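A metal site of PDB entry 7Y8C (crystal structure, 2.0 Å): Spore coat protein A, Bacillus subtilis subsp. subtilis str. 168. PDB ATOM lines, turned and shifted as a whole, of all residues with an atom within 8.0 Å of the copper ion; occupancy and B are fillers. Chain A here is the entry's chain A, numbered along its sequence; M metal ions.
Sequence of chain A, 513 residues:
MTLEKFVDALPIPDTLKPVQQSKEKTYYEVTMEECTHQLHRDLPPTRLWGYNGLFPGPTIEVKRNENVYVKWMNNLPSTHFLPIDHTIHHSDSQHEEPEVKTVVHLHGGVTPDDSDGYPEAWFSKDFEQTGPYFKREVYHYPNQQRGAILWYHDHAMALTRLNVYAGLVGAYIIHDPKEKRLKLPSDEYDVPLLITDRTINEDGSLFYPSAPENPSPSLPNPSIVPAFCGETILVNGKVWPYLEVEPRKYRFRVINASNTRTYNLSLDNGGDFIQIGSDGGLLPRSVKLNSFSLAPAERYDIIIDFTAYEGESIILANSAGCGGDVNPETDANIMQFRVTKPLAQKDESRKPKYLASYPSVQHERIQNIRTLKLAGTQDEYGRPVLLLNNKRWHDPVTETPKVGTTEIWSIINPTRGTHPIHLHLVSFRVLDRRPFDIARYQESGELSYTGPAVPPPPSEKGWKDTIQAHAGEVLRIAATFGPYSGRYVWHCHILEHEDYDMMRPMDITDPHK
Ile 494 touches the copper ion. SD of Met 502 touches the copper ion, at 3.3 Å. Of the 22 residues printed, 5 come within 4 Å of the copper ion.
The backbone carbonyl oxygen (O) of His 419 sits at hydrogen-bond distance from the backbone NH (N) of Ala 469. ND1 of His 419 lies close to SD of Met 502 (3.8 Å). The backbone NH of Met 502 is in hydrogen-bond range of the backbone carbonyl oxygen of His 497 (2.9 Å). The backbone NH (N) of Met 502 lies within hydrogen-bond range of the backbone carbonyl oxygen (O) of Leu 386 (3.1 Å). The backbone NH (N) of Cys 492 is in hydrogen-bond range of the backbone carbonyl oxygen (O) of Met 502 (3.1 Å). The backbone carbonyl oxygen of Pro 226 sits close to a ring nitrogen (NE2) of His 497, 3.1 Å away. The backbone NH (N) of Ile 494 lies close to the side-chain sulfur (SG) of Cys 492 (3.5 Å). A ring nitrogen (NE2) of His 419 sits at hydrogen-bond distance from the side-chain hydroxyl (OG1) of Thr 415, 2.9 Å away.
The copper ion is bound by ND1 of His 497 (2.1 Å), SG of Cys 492 (2.2 Å) and ND1 of His 419 (2.2 Å).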
ATOM      1  N   PRO A 226      19.335   5.104  13.526  1.00  0.00           N
ATOM      2  CA  PRO A 226      19.967   6.008  14.500  1.00  0.00           C
ATOM      3  C   PRO A 226      20.290   5.346  15.821  1.00  0.00           C
ATOM      4  O   PRO A 226      21.078   5.910  16.590  1.00  0.00           O
ATOM      5  CB  PRO A 226      18.935   7.124  14.674  1.00  0.00           C
ATOM      6  CG  PRO A 226      17.620   6.491  14.345  1.00  0.00           C
ATOM      7  CD  PRO A 226      17.922   5.453  13.266  1.00  0.00           C
ATOM      8  N   LEU A 374      27.575  19.254  19.987  1.00  0.00           N
ATOM      9  CA  LEU A 374      26.896  18.070  19.486  1.00  0.00           C
ATOM     10  C   LEU A 374      25.592  18.496  18.829  1.00  0.00           C
ATOM     11  O   LEU A 374      24.832  19.282  19.407  1.00  0.00           O
ATOM     12  CB  LEU A 374      26.612  17.069  20.604  1.00  0.00           C
ATOM     13  CG  LEU A 374      27.674  16.797  21.667  1.00  0.00           C
ATOM     14  CD1 LEU A 374      27.212  15.664  22.582  1.00  0.00           C
ATOM     15  CD2 LEU A 374      28.997  16.442  21.031  1.00  0.00           C
ATOM     16  N   LEU A 386      24.230  12.604  12.785  1.00  0.00           N
ATOM     17  CA  LEU A 386      24.765  13.194  14.005  1.00  0.00           C
ATOM     18  C   LEU A 386      26.190  13.679  13.761  1.00  0.00           C
ATOM     19  O   LEU A 386      27.001  12.968  13.166  1.00  0.00           O
ATOM     20  CB  LEU A 386      24.691  12.184  15.158  1.00  0.00           C
ATOM     21  CG  LEU A 386      23.243  12.137  15.691  1.00  0.00           C
ATOM     22  CD1 LEU A 386      22.968  10.946  16.581  1.00  0.00           C
ATOM     23  CD2 LEU A 386      22.911  13.430  16.426  1.00  0.00           C
ATOM     24  N   LEU A 387      26.494  14.899  14.218  1.00  0.00           N
ATOM     25  CA  LEU A 387      27.741  15.554  13.860  1.00  0.00           C
ATOM     26  C   LEU A 387      28.404  16.175  15.084  1.00  0.00           C
ATOM     27  O   LEU A 387      27.735  16.643  16.012  1.00  0.00           O
ATOM     28  CB  LEU A 387      27.534  16.627  12.791  1.00  0.00           C
ATOM     29  CG  LEU A 387      26.857  16.151  11.499  1.00  0.00           C
ATOM     30  CD1 LEU A 387      26.415  17.348  10.690  1.00  0.00           C
ATOM     31  CD2 LEU A 387      27.805  15.262  10.707  1.00  0.00           C
ATOM     32  N   LEU A 388      29.734  16.156  15.068  1.00  0.00           N
ATOM     33  CA  LEU A 388      30.531  16.885  16.037  1.00  0.00           C
ATOM     34  C   LEU A 388      30.900  18.244  15.439  1.00  0.00           C
ATOM     35  O   LEU A 388      31.464  18.304  14.345  1.00  0.00           O
ATOM     36  CB  LEU A 388      31.785  16.083  16.410  1.00  0.00           C
ATOM     37  CG  LEU A 388      31.571  14.669  16.956  1.00  0.00           C
ATOM     38  CD1 LEU A 388      32.886  13.946  17.129  1.00  0.00           C
ATOM     39  CD2 LEU A 388      30.805  14.724  18.275  1.00  0.00           C
ATOM     40  N   ASN A 413      25.717  19.977  24.618  1.00  0.00           N
ATOM     41  CA  ASN A 413      24.756  19.024  24.066  1.00  0.00           C
ATOM     42  C   ASN A 413      23.355  19.633  24.036  1.00  0.00           C
ATOM     43  O   ASN A 413      22.649  19.610  25.055  1.00  0.00           O
ATOM     44  CB  ASN A 413      24.769  17.727  24.883  1.00  0.00           C
ATOM     45  CG  ASN A 413      23.873  16.659  24.284  1.00  0.00           C
ATOM     46  OD1 ASN A 413      23.263  16.869  23.259  1.00  0.00           O
ATOM     47  ND2 ASN A 413      23.773  15.516  24.955  1.00  0.00           N
ATOM     48  N   THR A 415      21.036  18.330  22.030  1.00  0.00           N
ATOM     49  CA  THR A 415      20.195  17.295  21.463  1.00  0.00           C
ATOM     50  C   THR A 415      19.288  16.709  22.549  1.00  0.00           C
ATOM     51  O   THR A 415      19.376  17.055  23.727  1.00  0.00           O
ATOM     52  CB  THR A 415      21.047  16.201  20.804  1.00  0.00           C
ATOM     53  OG1 THR A 415      21.555  15.319  21.819  1.00  0.00           O
ATOM     54  CG2 THR A 415      22.217  16.833  20.030  1.00  0.00           C
ATOM     55  N   GLY A 417      19.158  13.530  23.636  1.00  0.00           N
ATOM     56  CA  GLY A 417      19.649  12.395  24.373  1.00  0.00           C
ATOM     57  C   GLY A 417      21.082  12.561  24.835  1.00  0.00           C
ATOM     58  O   GLY A 417      21.761  13.536  24.527  1.00  0.00           O
ATOM     59  N   THR A 418      21.526  11.571  25.599  1.00  0.00           N
ATOM     60  CA  THR A 418      22.901  11.519  26.086  1.00  0.00           C
ATOM     61  C   THR A 418      23.808  10.932  25.013  1.00  0.00           C
ATOM     62  O   THR A 418      23.414  10.036  24.268  1.00  0.00           O
ATOM     63  CB  THR A 418      22.987  10.662  27.340  1.00  0.00           C
ATOM     64  OG1 THR A 418      22.249  11.284  28.387  1.00  0.00           O
ATOM     65  CG2 THR A 418      24.431  10.476  27.771  1.00  0.00           C
ATOM     66  N   HIS A 419      25.035  11.447  24.945  1.00  0.00           N
ATOM     67  CA  HIS A 419      26.035  10.911  24.034  1.00  0.00           C
ATOM     68  C   HIS A 419      27.275  10.554  24.852  1.00  0.00           C
ATOM     69  O   HIS A 419      27.817  11.422  25.562  1.00  0.00           O
ATOM     70  CB  HIS A 419      26.390  11.912  22.925  1.00  0.00           C
ATOM     71  CG  HIS A 419      25.221  12.329  22.095  1.00  0.00           C
ATOM     72  ND1 HIS A 419      24.814  11.626  20.980  1.00  0.00           N
ATOM     73  CD2 HIS A 419      24.364  13.369  22.214  1.00  0.00           C
ATOM     74  CE1 HIS A 419      23.769  12.218  20.445  1.00  0.00           C
ATOM     75  NE2 HIS A 419      23.462  13.276  21.178  1.00  0.00           N
ATOM     76  N   PRO A 420      27.727   9.290  24.807  1.00  0.00           N
ATOM     77  CA  PRO A 420      28.953   8.906  25.511  1.00  0.00           C
ATOM     78  C   PRO A 420      30.170   9.222  24.662  1.00  0.00           C
ATOM     79  O   PRO A 420      30.447   8.526  23.684  1.00  0.00           O
ATOM     80  CB  PRO A 420      28.782   7.398  25.711  1.00  0.00           C
ATOM     81  CG  PRO A 420      27.914   6.970  24.517  1.00  0.00           C
ATOM     82  CD  PRO A 420      27.048   8.140  24.160  1.00  0.00           C
ATOM     83  N   ILE A 421      30.900  10.293  25.006  1.00  0.00           N
ATOM     84  CA  ILE A 421      31.952  10.815  24.136  1.00  0.00           C
ATOM     85  C   ILE A 421      33.259  10.156  24.519  1.00  0.00           C
ATOM     86  O   ILE A 421      33.597  10.070  25.701  1.00  0.00           O
ATOM     87  CB  ILE A 421      32.049  12.345  24.239  1.00  0.00           C
ATOM     88  CG1 ILE A 421      30.709  12.989  23.858  1.00  0.00           C
ATOM     89  CG2 ILE A 421      33.183  12.879  23.347  1.00  0.00           C
ATOM     90  CD1 ILE A 421      30.248  12.660  22.414  1.00  0.00           C
ATOM     91  N   ALA A 469      27.728  12.838  28.073  1.00  0.00           N
ATOM     92  CA  ALA A 469      27.321  14.227  27.939  1.00  0.00           C
ATOM     93  C   ALA A 469      25.805  14.240  27.821  1.00  0.00           C
ATOM     94  O   ALA A 469      25.256  13.868  26.779  1.00  0.00           O
ATOM     95  CB  ALA A 469      27.971  14.871  26.710  1.00  0.00           C
ATOM     96  N   HIS A 491      34.921  10.765  19.207  1.00  0.00           N
ATOM     97  CA  HIS A 491      33.635  10.380  18.637  1.00  0.00           C
ATOM     98  C   HIS A 491      32.638   9.971  19.724  1.00  0.00           C
ATOM     99  O   HIS A 491      33.010   9.644  20.846  1.00  0.00           O
ATOM    100  CB  HIS A 491      33.808   9.254  17.613  1.00  0.00           C
ATOM    101  CG  HIS A 491      34.421   8.009  18.173  1.00  0.00           C
ATOM    102  ND1 HIS A 491      33.663   6.974  18.702  1.00  0.00           N
ATOM    103  CD2 HIS A 491      35.717   7.608  18.278  1.00  0.00           C
ATOM    104  CE1 HIS A 491      34.471   6.015  19.123  1.00  0.00           C
ATOM    105  NE2 HIS A 491      35.724   6.370  18.875  1.00  0.00           N
ATOM    106  N   CYS A 492      31.355   9.986  19.363  1.00  0.00           N
ATOM    107  CA  CYS A 492      30.353   9.354  20.205  1.00  0.00           C
ATOM    108  C   CYS A 492      30.512   7.823  20.094  1.00  0.00           C
ATOM    109  O   CYS A 492      30.829   7.312  19.020  1.00  0.00           O
ATOM    110  CB  CYS A 492      28.954   9.788  19.788  1.00  0.00           C
ATOM    111  SG  CYS A 492      27.608   8.988  20.718  1.00  0.00           S
ATOM    112  N   HIS A 493      30.303   7.109  21.204  1.00  0.00           N
ATOM    113  CA  HIS A 493      30.471   5.653  21.168  1.00  0.00           C
ATOM    114  C   HIS A 493      29.161   4.879  21.086  1.00  0.00           C
ATOM    115  O   HIS A 493      29.153   3.664  21.302  1.00  0.00           O
ATOM    116  CB  HIS A 493      31.279   5.167  22.360  1.00  0.00           C
ATOM    117  CG  HIS A 493      32.203   4.031  22.009  1.00  0.00           C
ATOM    118  ND1 HIS A 493      31.748   2.735  21.828  1.00  0.00           N
ATOM    119  CD2 HIS A 493      33.528   4.001  21.762  1.00  0.00           C
ATOM    120  CE1 HIS A 493      32.762   1.962  21.493  1.00  0.00           C
ATOM    121  NE2 HIS A 493      33.860   2.707  21.451  1.00  0.00           N
ATOM    122  N   ILE A 494      28.051   5.557  20.806  1.00  0.00           N
ATOM    123  CA  ILE A 494      26.881   4.908  20.246  1.00  0.00           C
ATOM    124  C   ILE A 494      27.219   4.600  18.792  1.00  0.00           C
ATOM    125  O   ILE A 494      27.347   5.509  17.961  1.00  0.00           O
ATOM    126  CB  ILE A 494      25.629   5.792  20.361  1.00  0.00           C
ATOM    127  CG1 ILE A 494      25.232   5.924  21.844  1.00  0.00           C
ATOM    128  CG2 ILE A 494      24.486   5.284  19.460  1.00  0.00           C
ATOM    129  CD1 ILE A 494      24.200   7.037  22.139  1.00  0.00           C
ATOM    130  N   LEU A 495      27.436   3.312  18.479  1.00  0.00           N
ATOM    131  CA  LEU A 495      28.062   2.998  17.203  1.00  0.00           C
ATOM    132  C   LEU A 495      27.191   3.445  16.035  1.00  0.00           C
ATOM    133  O   LEU A 495      27.712   3.814  14.971  1.00  0.00           O
ATOM    134  CB  LEU A 495      28.393   1.502  17.120  1.00  0.00           C
ATOM    135  CG  LEU A 495      29.209   0.993  18.319  1.00  0.00           C
ATOM    136  CD1 LEU A 495      29.608  -0.496  18.133  1.00  0.00           C
ATOM    137  CD2 LEU A 495      30.437   1.869  18.584  1.00  0.00           C
ATOM    138  N   GLU A 496      25.869   3.435  16.210  1.00  0.00           N
ATOM    139  CA  GLU A 496      24.978   3.922  15.163  1.00  0.00           C
ATOM    140  C   GLU A 496      25.140   5.420  14.928  1.00  0.00           C
ATOM    141  O   GLU A 496      24.817   5.916  13.833  1.00  0.00           O
ATOM    142  CB  GLU A 496      23.523   3.579  15.507  1.00  0.00           C
ATOM    143  CG  GLU A 496      23.113   2.106  15.271  1.00  0.00           C
ATOM    144  CD  GLU A 496      23.724   1.119  16.284  1.00  0.00           C
ATOM    145  OE1 GLU A 496      24.022   1.543  17.442  1.00  0.00           O
ATOM    146  OE2 GLU A 496      23.897  -0.077  15.924  1.00  0.00           O
ATOM    147  N   HIS A 497      25.630   6.154  15.926  1.00  0.00           N
ATOM    148  CA  HIS A 497      25.953   7.574  15.767  1.00  0.00           C
ATOM    149  C   HIS A 497      27.346   7.751  15.165  1.00  0.00           C
ATOM    150  O   HIS A 497      27.544   8.552  14.245  1.00  0.00           O
ATOM    151  CB  HIS A 497      25.893   8.292  17.128  1.00  0.00           C
ATOM    152  CG  HIS A 497      24.523   8.366  17.721  1.00  0.00           C
ATOM    153  ND1 HIS A 497      24.261   9.049  18.900  1.00  0.00           N
ATOM    154  CD2 HIS A 497      23.334   7.845  17.317  1.00  0.00           C
ATOM    155  CE1 HIS A 497      22.980   8.945  19.189  1.00  0.00           C
ATOM    156  NE2 HIS A 497      22.395   8.215  18.249  1.00  0.00           N
ATOM    157  N   GLU A 498      28.315   7.019  15.720  1.00  0.00           N
ATOM    158  CA  GLU A 498      29.696   7.048  15.259  1.00  0.00           C
ATOM    159  C   GLU A 498      29.792   6.858  13.752  1.00  0.00           C
ATOM    160  O   GLU A 498      30.500   7.607  13.066  1.00  0.00           O
ATOM    161  CB  GLU A 498      30.520   5.976  15.987  1.00  0.00           C
ATOM    162  CG  GLU A 498      31.949   5.808  15.461  1.00  0.00           C
ATOM    163  CD  GLU A 498      32.755   4.718  16.210  1.00  0.00           C
ATOM    164  OE1 GLU A 498      32.405   4.389  17.364  1.00  0.00           O
ATOM    165  OE2 GLU A 498      33.741   4.220  15.647  1.00  0.00           O
ATOM    166  N   MET A 502      29.236  10.827  13.581  1.00  0.00           N
ATOM    167  CA  MET A 502      29.614  11.528  14.807  1.00  0.00           C
ATOM    168  C   MET A 502      31.017  11.144  15.278  1.00  0.00           C
ATOM    169  O   MET A 502      31.222  10.618  16.372  1.00  0.00           O
ATOM    170  CB  MET A 502      28.590  11.254  15.896  1.00  0.00           C
ATOM    171  CG  MET A 502      28.366  12.415  16.824  1.00  0.00           C
ATOM    172  SD  MET A 502      27.005  12.107  17.964  1.00  0.00           S
ATOM    173  CE  MET A 502      27.288  13.461  19.098  1.00  0.00           C
HETATM  174 CU    CU M   1      25.780   9.913  20.061  1.00  0.00          CU
